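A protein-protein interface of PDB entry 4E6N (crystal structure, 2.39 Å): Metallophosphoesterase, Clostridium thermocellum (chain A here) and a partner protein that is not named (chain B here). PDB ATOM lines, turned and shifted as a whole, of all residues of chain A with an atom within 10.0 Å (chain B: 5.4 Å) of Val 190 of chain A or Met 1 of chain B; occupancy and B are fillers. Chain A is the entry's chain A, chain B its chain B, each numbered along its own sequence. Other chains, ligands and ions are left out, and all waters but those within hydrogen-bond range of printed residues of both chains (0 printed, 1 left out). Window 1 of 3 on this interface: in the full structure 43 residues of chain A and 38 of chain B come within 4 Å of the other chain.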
ATOM      1  N   ALA A 182      14.787  16.024 -14.580  1.00  0.00           N
ATOM      2  CA  ALA A 182      14.449  17.115 -15.486  1.00  0.00           C
ATOM      3  C   ALA A 182      15.084  16.856 -16.849  1.00  0.00           C
ATOM      4  O   ALA A 182      14.434  16.977 -17.885  1.00  0.00           O
ATOM      5  CB  ALA A 182      14.893  18.456 -14.913  1.00  0.00           C
ATOM      6  N   VAL A 183      16.351  16.465 -16.840  1.00  0.00           N
ATOM      7  CA  VAL A 183      17.030  16.061 -18.070  1.00  0.00           C
ATOM      8  C   VAL A 183      16.349  14.837 -18.681  1.00  0.00           C
ATOM      9  O   VAL A 183      16.189  14.746 -19.892  1.00  0.00           O
ATOM     10  CB  VAL A 183      18.518  15.754 -17.809  1.00  0.00           C
ATOM     11  CG1 VAL A 183      19.208  15.253 -19.088  1.00  0.00           C
ATOM     12  CG2 VAL A 183      19.215  16.988 -17.258  1.00  0.00           C
ATOM     13  N   GLY A 184      15.933  13.905 -17.831  1.00  0.00           N
ATOM     14  CA  GLY A 184      15.308  12.674 -18.283  1.00  0.00           C
ATOM     15  C   GLY A 184      13.947  12.803 -18.949  1.00  0.00           C
ATOM     16  O   GLY A 184      13.683  12.117 -19.946  1.00  0.00           O
ATOM     17  N   ILE A 185      13.070  13.648 -18.404  1.00  0.00           N
ATOM     18  CA  ILE A 185      11.757  13.844 -19.026  1.00  0.00           C
ATOM     19  C   ILE A 185      11.872  14.687 -20.303  1.00  0.00           C
ATOM     20  O   ILE A 185      11.326  14.326 -21.343  1.00  0.00           O
ATOM     21  CB  ILE A 185      10.677  14.404 -18.033  1.00  0.00           C
ATOM     22  CG1 ILE A 185       9.298  14.411 -18.688  1.00  0.00           C
ATOM     23  CG2 ILE A 185      11.015  15.805 -17.536  1.00  0.00           C
ATOM     24  CD1 ILE A 185       8.814  13.053 -19.148  1.00  0.00           C
ATOM     25  N   SER A 186      12.624  15.782 -20.234  1.00  0.00           N
ATOM     26  CA  SER A 186      12.809  16.647 -21.398  1.00  0.00           C
ATOM     27  C   SER A 186      13.538  15.893 -22.502  1.00  0.00           C
ATOM     28  O   SER A 186      13.141  15.948 -23.662  1.00  0.00           O
ATOM     29  CB  SER A 186      13.557  17.928 -21.030  1.00  0.00           C
ATOM     30  OG  SER A 186      14.902  17.674 -20.698  1.00  0.00           O
ATOM     31  N   GLY A 187      14.583  15.164 -22.126  1.00  0.00           N
ATOM     32  CA  GLY A 187      15.328  14.351 -23.067  1.00  0.00           C
ATOM     33  C   GLY A 187      14.517  13.248 -23.727  1.00  0.00           C
ATOM     34  O   GLY A 187      14.597  13.072 -24.939  1.00  0.00           O
ATOM     35  N   ARG A 188      13.737  12.494 -22.955  1.00  0.00           N
ATOM     36  CA  ARG A 188      13.015  11.372 -23.548  1.00  0.00           C
ATOM     37  C   ARG A 188      11.912  11.856 -24.470  1.00  0.00           C
ATOM     38  O   ARG A 188      11.638  11.238 -25.490  1.00  0.00           O
ATOM     39  CB  ARG A 188      12.454  10.428 -22.493  1.00  0.00           C
ATOM     40  CG  ARG A 188      13.470   9.434 -21.939  1.00  0.00           C
ATOM     41  CD  ARG A 188      12.851   8.597 -20.838  1.00  0.00           C
ATOM     42  NE  ARG A 188      12.442   9.430 -19.711  1.00  0.00           N
ATOM     43  CZ  ARG A 188      11.309   9.260 -19.031  1.00  0.00           C
ATOM     44  NH1 ARG A 188      10.480   8.281 -19.370  1.00  0.00           N
ATOM     45  NH2 ARG A 188      10.996  10.067 -18.021  1.00  0.00           N
ATOM     46  N   VAL A 189      11.307  12.982 -24.121  1.00  0.00           N
ATOM     47  CA  VAL A 189      10.175  13.474 -24.880  1.00  0.00           C
ATOM     48  C   VAL A 189      10.572  14.060 -26.236  1.00  0.00           C
ATOM     49  O   VAL A 189       9.950  13.730 -27.253  1.00  0.00           O
ATOM     50  CB  VAL A 189       9.345  14.496 -24.072  1.00  0.00           C
ATOM     51  CG1 VAL A 189       8.395  15.262 -24.989  1.00  0.00           C
ATOM     52  CG2 VAL A 189       8.594  13.782 -22.956  1.00  0.00           C
ATOM     53  N   VAL A 190      11.590  14.920 -26.271  1.00  0.00           N
ATOM     54  CA  VAL A 190      11.933  15.558 -27.544  1.00  0.00           C
ATOM     55  C   VAL A 190      12.714  14.615 -28.460  1.00  0.00           C
ATOM     56  O   VAL A 190      12.621  14.699 -29.688  1.00  0.00           O
ATOM     57  CB  VAL A 190      12.716  16.867 -27.364  1.00  0.00           C
ATOM     58  CG1 VAL A 190      11.886  17.867 -26.579  1.00  0.00           C
ATOM     59  CG2 VAL A 190      14.097  16.600 -26.699  1.00  0.00           C
ATOM     60  N   LEU A 191      13.482  13.716 -27.865  1.00  0.00           N
ATOM     61  CA  LEU A 191      14.262  12.788 -28.666  1.00  0.00           C
ATOM     62  C   LEU A 191      13.372  11.755 -29.357  1.00  0.00           C
ATOM     63  O   LEU A 191      13.649  11.374 -30.485  1.00  0.00           O
ATOM     64  CB  LEU A 191      15.377  12.142 -27.840  1.00  0.00           C
ATOM     65  CG  LEU A 191      16.583  13.058 -27.543  1.00  0.00           C
ATOM     66  CD1 LEU A 191      17.625  12.380 -26.634  1.00  0.00           C
ATOM     67  CD2 LEU A 191      17.254  13.560 -28.821  1.00  0.00           C
ATOM     68  N   ASP A 192      12.298  11.326 -28.688  1.00  0.00           N
ATOM     69  CA  ASP A 192      11.328  10.415 -29.297  1.00  0.00           C
ATOM     70  C   ASP A 192      10.549  11.115 -30.392  1.00  0.00           C
ATOM     71  O   ASP A 192      10.229  10.514 -31.405  1.00  0.00           O
ATOM     72  CB  ASP A 192      10.339   9.855 -28.273  1.00  0.00           C
ATOM     73  CG  ASP A 192      10.955   8.798 -27.367  1.00  0.00           C
ATOM     74  OD1 ASP A 192      11.918   8.122 -27.783  1.00  0.00           O
ATOM     75  OD2 ASP A 192      10.463   8.640 -26.233  1.00  0.00           O
ATOM     76  N   GLU A 193      10.227  12.385 -30.172  1.00  0.00           N
ATOM     77  CA  GLU A 193       9.508  13.139 -31.169  1.00  0.00           C
ATOM     78  C   GLU A 193      10.410  13.409 -32.377  1.00  0.00           C
ATOM     79  O   GLU A 193       9.947  13.396 -33.525  1.00  0.00           O
ATOM     80  CB  GLU A 193       8.942  14.434 -30.590  1.00  0.00           C
ATOM     81  CG  GLU A 193       8.156  15.276 -31.613  1.00  0.00           C
ATOM     82  CD  GLU A 193       6.893  14.591 -32.153  1.00  0.00           C
ATOM     83  OE1 GLU A 193       6.470  14.954 -33.275  1.00  0.00           O
ATOM     84  OE2 GLU A 193       6.315  13.709 -31.468  1.00  0.00           O
ATOM     85  N   ALA A 194      11.695  13.626 -32.117  1.00  0.00           N
ATOM     86  CA  ALA A 194      12.668  13.836 -33.181  1.00  0.00           C
ATOM     87  C   ALA A 194      12.772  12.613 -34.079  1.00  0.00           C
ATOM     88  O   ALA A 194      12.773  12.720 -35.300  1.00  0.00           O
ATOM     89  CB  ALA A 194      14.036  14.167 -32.600  1.00  0.00           C
ATOM     90  N   VAL A 195      12.855  11.446 -33.465  1.00  0.00           N
ATOM     91  CA  VAL A 195      12.938  10.203 -34.213  1.00  0.00           C
ATOM     92  C   VAL A 195      11.705   9.994 -35.097  1.00  0.00           C
ATOM     93  O   VAL A 195      11.810   9.613 -36.259  1.00  0.00           O
ATOM     94  CB  VAL A 195      13.118   9.006 -33.259  1.00  0.00           C
ATOM     95  CG1 VAL A 195      12.883   7.687 -33.986  1.00  0.00           C
ATOM     96  CG2 VAL A 195      14.499   9.039 -32.647  1.00  0.00           C
ATOM     97  N   LYS A 196      10.539  10.273 -34.531  1.00  0.00           N
ATOM     98  CA  LYS A 196       9.275  10.127 -35.226  1.00  0.00           C
ATOM     99  C   LYS A 196       9.150  11.066 -36.448  1.00  0.00           C
ATOM    100  O   LYS A 196       8.692  10.647 -37.514  1.00  0.00           O
ATOM    101  CB  LYS A 196       8.134  10.339 -34.225  1.00  0.00           C
ATOM    102  CG  LYS A 196       6.726  10.266 -34.793  1.00  0.00           C
ATOM    103  CD  LYS A 196       5.722  10.629 -33.709  1.00  0.00           C
ATOM    104  CE  LYS A 196       4.291  10.442 -34.176  1.00  0.00           C
ATOM    105  NZ  LYS A 196       3.327  10.594 -33.043  1.00  0.00           N
ATOM    106  N   LEU A 197       9.570  12.320 -36.299  1.00  0.00           N
ATOM    107  CA  LEU A 197       9.501  13.269 -37.410  1.00  0.00           C
ATOM    108  C   LEU A 197      10.470  12.915 -38.540  1.00  0.00           C
ATOM    109  O   LEU A 197      10.137  13.046 -39.715  1.00  0.00           O
ATOM    110  CB  LEU A 197       9.742  14.697 -36.927  1.00  0.00           C
ATOM    111  CG  LEU A 197       8.670  15.237 -35.977  1.00  0.00           C
ATOM    112  CD1 LEU A 197       9.213  16.458 -35.242  1.00  0.00           C
ATOM    113  CD2 LEU A 197       7.312  15.540 -36.703  1.00  0.00           C
ATOM    114  N   LEU A 198      11.664  12.467 -38.173  1.00  0.00           N
ATOM    115  CA  LEU A 198      12.683  12.116 -39.150  1.00  0.00           C
ATOM    116  C   LEU A 198      12.265  10.867 -39.920  1.00  0.00           C
ATOM    117  O   LEU A 198      12.470  10.776 -41.124  1.00  0.00           O
ATOM    118  CB  LEU A 198      14.029  11.896 -38.455  1.00  0.00           C
ATOM    119  CG  LEU A 198      14.737  13.189 -38.057  1.00  0.00           C
ATOM    120  CD1 LEU A 198      15.784  12.919 -36.969  1.00  0.00           C
ATOM    121  CD2 LEU A 198      15.384  13.829 -39.281  1.00  0.00           C
ATOM    122  N   LEU A 225      20.649  11.562 -40.236  1.00  0.00           N
ATOM    123  CA  LEU A 225      20.022  12.294 -39.142  1.00  0.00           C
ATOM    124  C   LEU A 225      19.166  11.360 -38.311  1.00  0.00           C
ATOM    125  O   LEU A 225      19.227  11.372 -37.076  1.00  0.00           O
ATOM    126  CB  LEU A 225      19.185  13.468 -39.672  1.00  0.00           C
ATOM    127  CG  LEU A 225      20.030  14.627 -40.221  1.00  0.00           C
ATOM    128  CD1 LEU A 225      19.176  15.688 -40.872  1.00  0.00           C
ATOM    129  CD2 LEU A 225      20.886  15.242 -39.109  1.00  0.00           C
ATOM    130  N   ARG A 228      21.454   9.063 -36.224  1.00  0.00           N
ATOM    131  CA  ARG A 228      21.998   9.838 -35.131  1.00  0.00           C
ATOM    132  C   ARG A 228      20.993  10.030 -33.986  1.00  0.00           C
ATOM    133  O   ARG A 228      21.287   9.717 -32.838  1.00  0.00           O
ATOM    134  CB  ARG A 228      22.457  11.191 -35.676  1.00  0.00           C
ATOM    135  CG  ARG A 228      22.742  12.227 -34.614  1.00  0.00           C
ATOM    136  CD  ARG A 228      23.367  13.474 -35.231  1.00  0.00           C
ATOM    137  NE  ARG A 228      23.737  14.439 -34.203  1.00  0.00           N
ATOM    138  CZ  ARG A 228      24.784  14.304 -33.395  1.00  0.00           C
ATOM    139  NH1 ARG A 228      25.577  13.247 -33.504  1.00  0.00           N
ATOM    140  NH2 ARG A 228      25.045  15.228 -32.478  1.00  0.00           N
ATOM    141  N   PHE A 229      19.796  10.520 -34.306  1.00  0.00           N
ATOM    142  CA  PHE A 229      18.824  10.823 -33.271  1.00  0.00           C
ATOM    143  C   PHE A 229      18.251   9.559 -32.666  1.00  0.00           C
ATOM    144  O   PHE A 229      17.861   9.547 -31.503  1.00  0.00           O
ATOM    145  CB  PHE A 229      17.735  11.777 -33.774  1.00  0.00           C
ATOM    146  CG  PHE A 229      18.147  13.214 -33.734  1.00  0.00           C
ATOM    147  CD1 PHE A 229      18.979  13.738 -34.712  1.00  0.00           C
ATOM    148  CD2 PHE A 229      17.732  14.036 -32.705  1.00  0.00           C
ATOM    149  CE1 PHE A 229      19.375  15.055 -34.668  1.00  0.00           C
ATOM    150  CE2 PHE A 229      18.120  15.362 -32.662  1.00  0.00           C
ATOM    151  CZ  PHE A 229      18.943  15.875 -33.641  1.00  0.00           C
ATOM    152  N   THR A 230      18.244   8.482 -33.435  1.00  0.00           N
ATOM    153  CA  THR A 230      17.851   7.186 -32.876  1.00  0.00           C
ATOM    154  C   THR A 230      18.853   6.761 -31.790  1.00  0.00           C
ATOM    155  O   THR A 230      18.485   6.252 -30.732  1.00  0.00           O
ATOM    156  CB  THR A 230      17.728   6.113 -33.975  1.00  0.00           C
ATOM    157  OG1 THR A 230      16.635   6.458 -34.832  1.00  0.00           O
ATOM    158  CG2 THR A 230      17.468   4.731 -33.378  1.00  0.00           C
ATOM    159  N   ARG A 232      20.882   8.974 -30.086  1.00  0.00           N
ATOM    160  CA  ARG A 232      20.729   9.904 -28.967  1.00  0.00           C
ATOM    161  C   ARG A 232      19.572   9.457 -28.086  1.00  0.00           C
ATOM    162  O   ARG A 232      19.673   9.477 -26.855  1.00  0.00           O
ATOM    163  CB  ARG A 232      20.521  11.347 -29.425  1.00  0.00           C
ATOM    164  CG  ARG A 232      21.666  11.956 -30.221  1.00  0.00           C
ATOM    165  CD  ARG A 232      21.351  13.408 -30.620  1.00  0.00           C
ATOM    166  NE  ARG A 232      21.408  14.297 -29.461  1.00  0.00           N
ATOM    167  CZ  ARG A 232      20.990  15.561 -29.436  1.00  0.00           C
ATOM    168  NH1 ARG A 232      20.453  16.129 -30.506  1.00  0.00           N
ATOM    169  NH2 ARG A 232      21.088  16.262 -28.316  1.00  0.00           N
ATOM    170  N   SER A 233      18.494   9.005 -28.720  1.00  0.00           N
ATOM    171  CA  SER A 233      17.315   8.517 -27.993  1.00  0.00           C
ATOM    172  C   SER A 233      17.558   7.270 -27.123  1.00  0.00           C
ATOM    173  O   SER A 233      17.031   7.157 -26.003  1.00  0.00           O
ATOM    174  CB  SER A 233      16.176   8.230 -28.974  1.00  0.00           C
ATOM    175  OG  SER A 233      15.065   7.715 -28.285  1.00  0.00           O
ATOM    176  N   MET A 236      19.594   8.254 -24.087  1.00  0.00           N
ATOM    177  CA  MET A 236      18.796   9.001 -23.132  1.00  0.00           C
ATOM    178  C   MET A 236      17.969   8.041 -22.314  1.00  0.00           C
ATOM    179  O   MET A 236      17.810   8.223 -21.106  1.00  0.00           O
ATOM    180  CB  MET A 236      17.894  10.022 -23.835  1.00  0.00           C
ATOM    181  CG  MET A 236      16.923  10.752 -22.901  1.00  0.00           C
ATOM    182  SD  MET A 236      17.752  11.755 -21.635  1.00  0.00           S
ATOM    183  CE  MET A 236      18.730  12.836 -22.670  1.00  0.00           C
ATOM    184  N   GLU A 363      24.715  11.340 -23.036  1.00  0.00           N
ATOM    185  CA  GLU A 363      25.268  11.114 -24.369  1.00  0.00           C
ATOM    186  C   GLU A 363      26.802  11.022 -24.436  1.00  0.00           C
ATOM    187  O   GLU A 363      27.367  11.045 -25.524  1.00  0.00           O
ATOM    188  CB  GLU A 363      24.798  12.217 -25.319  1.00  0.00           C
ATOM    189  CG  GLU A 363      23.295  12.309 -25.489  1.00  0.00           C
ATOM    190  CD  GLU A 363      22.911  13.263 -26.592  1.00  0.00           C
ATOM    191  OE1 GLU A 363      23.585  13.249 -27.643  1.00  0.00           O
ATOM    192  OE2 GLU A 363      21.948  14.033 -26.405  1.00  0.00           O
ATOM    193  N   MET B   1      13.300  21.613 -28.000  1.00  0.00           N
ATOM    194  CA  MET B   1      14.380  21.222 -28.894  1.00  0.00           C
ATOM    195  C   MET B   1      13.835  21.250 -30.314  1.00  0.00           C
ATOM    196  O   MET B   1      14.587  21.335 -31.289  1.00  0.00           O
ATOM    197  CB  MET B   1      14.915  19.814 -28.545  1.00  0.00           C
ATOM    198  CG  MET B   1      16.206  19.424 -29.278  1.00  0.00           C
ATOM    199  SD  MET B   1      16.748  17.699 -29.064  1.00  0.00           S
ATOM    200  CE  MET B   1      15.649  16.853 -30.178  1.00  0.00           C
ATOM    201  N   ILE B   2      12.513  21.194 -30.418  1.00  0.00           N
ATOM    202  CA  ILE B   2      11.859  21.118 -31.711  1.00  0.00           C
ATOM    203  C   ILE B   2      10.831  22.213 -31.910  1.00  0.00           C
ATOM    204  O   ILE B   2      10.069  22.534 -31.007  1.00  0.00           O
ATOM    205  CB  ILE B   2      11.172  19.762 -31.909  1.00  0.00           C
ATOM    206  CG1 ILE B   2      12.150  18.629 -31.607  1.00  0.00           C
ATOM    207  CG2 ILE B   2      10.659  19.639 -33.323  1.00  0.00           C
ATOM    208  CD1 ILE B   2      11.536  17.258 -31.741  1.00  0.00           C
ATOM    209  N   LEU B   3      10.845  22.785 -33.109  1.00  0.00           N
ATOM    210  CA  LEU B   3       9.823  23.706 -33.576  1.00  0.00           C
ATOM    211  C   LEU B   3       9.255  23.145 -34.875  1.00  0.00           C
ATOM    212  O   LEU B   3      10.008  22.851 -35.806  1.00  0.00           O
ATOM    213  CB  LEU B   3      10.452  25.067 -33.876  1.00  0.00           C
ATOM    214  CG  LEU B   3       9.552  26.004 -34.686  1.00  0.00           C
ATOM    215  CD1 LEU B   3       8.280  26.333 -33.919  1.00  0.00           C
ATOM    216  CD2 LEU B   3      10.283  27.292 -35.110  1.00  0.00           C
ATOM    217  N   LEU B  52      12.254  22.291 -37.281  1.00  0.00           N
ATOM    218  CA  LEU B  52      13.533  22.870 -36.900  1.00  0.00           C
ATOM    219  C   LEU B  52      14.035  22.142 -35.644  1.00  0.00           C
ATOM    220  O   LEU B  52      13.422  22.201 -34.570  1.00  0.00           O
ATOM    221  CB  LEU B  52      13.389  24.385 -36.676  1.00  0.00           C
ATOM    222  CG  LEU B  52      14.639  25.147 -36.235  1.00  0.00           C
ATOM    223  CD1 LEU B  52      15.764  24.895 -37.201  1.00  0.00           C
ATOM    224  CD2 LEU B  52      14.365  26.621 -36.116  1.00  0.00           C
ATOM    225  N   LEU B  53      15.149  21.445 -35.805  1.00  0.00           N
ATOM    226  CA  LEU B  53      15.700  20.554 -34.789  1.00  0.00           C
ATOM    227  C   LEU B  53      17.032  21.073 -34.233  1.00  0.00           C
ATOM    228  O   LEU B  53      17.993  21.245 -34.988  1.00  0.00           O
ATOM    229  CB  LEU B  53      15.959  19.209 -35.452  1.00  0.00           C
ATOM    230  CG  LEU B  53      15.677  17.908 -34.728  1.00  0.00           C
ATOM    231  CD1 LEU B  53      14.212  17.815 -34.387  1.00  0.00           C
ATOM    232  CD2 LEU B  53      16.067  16.767 -35.641  1.00  0.00           C
ATOM    233  N   LEU B  54      17.099  21.315 -32.925  1.00  0.00           N
ATOM    234  CA  LEU B  54      18.359  21.721 -32.295  1.00  0.00           C
ATOM    235  C   LEU B  54      19.242  20.500 -32.050  1.00  0.00           C
ATOM    236  O   LEU B  54      18.758  19.447 -31.637  1.00  0.00           O
ATOM    237  CB  LEU B  54      18.122  22.445 -30.975  1.00  0.00           C
ATOM    238  CG  LEU B  54      17.351  23.769 -30.956  1.00  0.00           C
ATOM    239  CD1 LEU B  54      17.240  24.262 -29.516  1.00  0.00           C
ATOM    240  CD2 LEU B  54      18.000  24.832 -31.830  1.00  0.00           C
ATOM    241  N   PRO B  82      20.438  20.897 -23.986  1.00  0.00           N
ATOM    242  CA  PRO B  82      20.300  20.302 -25.323  1.00  0.00           C
ATOM    243  C   PRO B  82      18.868  19.873 -25.680  1.00  0.00           C
ATOM    244  O   PRO B  82      18.637  19.518 -26.834  1.00  0.00           O
ATOM    245  CB  PRO B  82      21.195  19.040 -25.256  1.00  0.00           C
ATOM    246  CG  PRO B  82      22.060  19.234 -24.070  1.00  0.00           C
ATOM    247  CD  PRO B  82      21.255  20.049 -23.099  1.00  0.00           C
ATOM    248  N   TYR B  83      17.940  19.898 -24.727  1.00  0.00           N
ATOM    249  CA  TYR B  83      16.639  19.245 -24.922  1.00  0.00           C
ATOM    250  C   TYR B  83      15.418  20.169 -24.817  1.00  0.00           C
ATOM    251  O   TYR B  83      14.281  19.712 -24.825  1.00  0.00           O
ATOM    252  CB  TYR B  83      16.500  18.073 -23.938  1.00  0.00           C
ATOM    253  CG  TYR B  83      17.750  17.223 -23.904  1.00  0.00           C
ATOM    254  CD1 TYR B  83      18.155  16.510 -25.034  1.00  0.00           C
ATOM    255  CD2 TYR B  83      18.546  17.154 -22.756  1.00  0.00           C
ATOM    256  CE1 TYR B  83      19.310  15.757 -25.020  1.00  0.00           C
ATOM    257  CE2 TYR B  83      19.705  16.387 -22.736  1.00  0.00           C
ATOM    258  CZ  TYR B  83      20.083  15.694 -23.874  1.00  0.00           C
ATOM    259  OH  TYR B  83      21.233  14.928 -23.881  1.00  0.00           O
ATOM    260  N   VAL B  84      15.655  21.466 -24.727  1.00  0.00           N
ATOM    261  CA  VAL B  84      14.569  22.386 -24.495  1.00  0.00           C
ATOM    262  C   VAL B  84      14.540  23.527 -25.512  1.00  0.00           C
ATOM    263  O   VAL B  84      15.519  23.817 -26.199  1.00  0.00           O
ATOM    264  CB  VAL B  84      14.622  22.967 -23.057  1.00  0.00           C
ATOM    265  CG1 VAL B  84      14.530  21.856 -22.042  1.00  0.00           C
ATOM    266  CG2 VAL B  84      15.893  23.787 -22.850  1.00  0.00           C
ATOM    267  N   SER B  85      13.395  24.172 -25.607  1.00  0.00           N
ATOM    268  CA  SER B  85      13.285  25.352 -26.437  1.00  0.00           C
ATOM    269  C   SER B  85      13.659  26.572 -25.617  1.00  0.00           C
ATOM    270  O   SER B  85      12.796  27.283 -25.102  1.00  0.00           O
ATOM    271  CB  SER B  85      11.875  25.480 -27.019  1.00  0.00           C
ATOM    272  OG  SER B  85      11.660  24.452 -27.971  1.00  0.00           O
ATOM    273  N   MET B  89      16.822  28.228 -29.431  1.00  0.00           N
ATOM    274  CA  MET B  89      15.800  28.062 -30.463  1.00  0.00           C
ATOM    275  C   MET B  89      15.561  29.371 -31.239  1.00  0.00           C
ATOM    276  O   MET B  89      15.515  29.367 -32.467  1.00  0.00           O
ATOM    277  CB  MET B  89      14.497  27.516 -29.860  1.00  0.00           C
ATOM    278  CG  MET B  89      13.395  27.297 -30.875  1.00  0.00           C
ATOM    279  SD  MET B  89      13.855  26.072 -32.122  1.00  0.00           S
ATOM    280  CE  MET B  89      13.739  24.560 -31.160  1.00  0.00           C
ATOM    281  N   MET B 123       8.150  22.553 -28.502  1.00  0.00           N
ATOM    282  CA  MET B 123       8.314  21.526 -27.475  1.00  0.00           C
ATOM    283  C   MET B 123       9.210  21.933 -26.326  1.00  0.00           C
ATOM    284  O   MET B 123      10.181  22.672 -26.510  1.00  0.00           O
ATOM    285  CB  MET B 123       8.880  20.268 -28.100  1.00  0.00           C
ATOM    286  CG  MET B 123       8.095  19.848 -29.319  1.00  0.00           C
ATOM    287  SD  MET B 123       8.186  18.087 -29.521  1.00  0.00           S
ATOM    288  CE  MET B 123       6.942  17.574 -28.352  1.00  0.00           C
ATOM    289  N   MET B 124       8.869  21.433 -25.143  1.00  0.00           N
ATOM    290  CA  MET B 124       9.737  21.529 -23.975  1.00  0.00           C
ATOM    291  C   MET B 124      10.209  22.960 -23.716  1.00  0.00           C
ATOM    292  O   MET B 124      11.385  23.228 -23.605  1.00  0.00           O
ATOM    293  CB  MET B 124      10.921  20.571 -24.121  1.00  0.00           C
ATOM    294  CG  MET B 124      10.783  19.291 -23.274  1.00  0.00           C
ATOM    295  SD  MET B 124       9.110  18.597 -23.261  1.00  0.00           S
ATOM    296  CE  MET B 124       9.145  17.664 -21.729  1.00  0.00           C
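The backbone NH of Leu 54 of chain B sits at hydrogen-bond distance from the backbone carbonyl oxygen of Met 1 of chain B, at 3.0 Å. O of Ile 2 of chain B is in hydrogen-bond range of N of Met 123 of chain B, 3.2 Å away. OG of Ser 85 of chain B sits at hydrogen-bond distance from O of Met 123 of chain B, at 2.7 Å. The side-chain hydroxyl (OG) of Ser 186 of chain A sits at hydrogen-bond distance from the backbone carbonyl oxygen (O) of Ala 182 of chain A, 2.9 Å away. The backbone NH (N) of Met 1 of chain B sits at hydrogen-bond distance from the side-chain hydroxyl (OG) of Ser 85 of chain B, 3.3 Å away. O of Val 183 of chain A sits at hydrogen-bond distance from OG of Ser 186 of chain A, at 3.3 Å.
Among the printed residues, merely in contact across the chains: Val 183 of chain A with Tyr 83 of chain B (3.9 Å), Ser 186 of chain A with Tyr 83 of chain B (3.6 Å), Ser 186 of chain A with Met 124 of chain B (3.8 Å), Gly 187 of chain A with Tyr 83 of chain B (3.8 Å), Val 189 of chain A with Met 124 of chain B (3.8 Å), Val 190 of chain A with Met 1 of chain B (3.7 Å), Val 190 of chain A with Ile 2 of chain B (3.5 Å), Val 190 of chain A with Tyr 83 of chain B (3.5 Å), Val 190 of chain A with Met 124 of chain B (3.8 Å), Leu 191 of chain A with Met 1 of chain B (3.9 Å), Glu 193 of chain A with Ile 2 of chain B (3.9 Å), Glu 193 of chain A with Met 123 of chain B (3.5 Å), Ala 194 of chain A with Met 1 of chain B (3.96 Å), Ala 194 of chain A with Ile 2 of chain B (3.7 Å), Leu 197 of chain A with Ile 2 of chain B (3.99 Å), Phe 229 of chain A with Met 1 of chain B (3.8 Å), Phe 229 of chain A with Leu 53 of chain B (3.6 Å), Arg 232 of chain A with Leu 54 of chain B (3.9 Å), Arg 232 of chain A with Tyr 83 of chain B (3.8 Å) and Met 236 of chain A with Tyr 83 of chain B (3.4 Å).
The side-chain carboxylate (OE2) of Glu 363 of chain A sits at hydrogen-bond distance from the side-chain hydroxyl (OH) of Tyr 83 of chain B (2.8 Å).
Of chain B, only Met 1, Ile 2, Tyr 83 and Met 124 come within 4 Å of Val 190 of chain A. Met 1 of chain B touches just these residues of chain A: Val 190 (3.7 Å), Leu 191 (3.9 Å), Ala 194 (3.96 Å) and Phe 229 (3.8 Å). Leu 53 of chain B touches just one residue of chain A: Phe 229 (3.6 Å). Leu 54 of chain B touches one residue of chain A. Of the printed residues of chain B, Glu 193 of chain A touches Ile 2 (3.9 Å) and Met 123 (3.5 Å). Of the printed residues of chain B, Ser 186 of chain A touches Tyr 83 and Met 124. Asp 192 of chain A touches none of the printed residues of chain B. The nearest residue of chain B that does not touch Val 190 of chain A is Met 123 of chain B (4.1 Å). The nearest printed residue of chain A that does not touch Met 124 of chain B is Ile 185 of chain A (4.01 Å).
Of the 25 printed residues of chain A, 13 touch a printed residue of chain B. Hydrophobic or aromatic side chains of chain A within 4 Å of the printed part of chain B: Val 183, Val 189, Val 190, Leu 191, Ala 194, Leu 197, Phe 229 and Met 236. Hydrophobic or aromatic side chains of chain B within 4 Å of the printed part of chain A: Met 1, Ile 2, Leu 53, Tyr 83, Met 123 and Met 124. Along chain B the printed residues that touch a printed residue of chain A span positions 1 to 124. Among the printed residues, no Asp or Glu carboxylate lies within 4 Å of a Lys or Arg side-chain nitrogen of the other chain.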
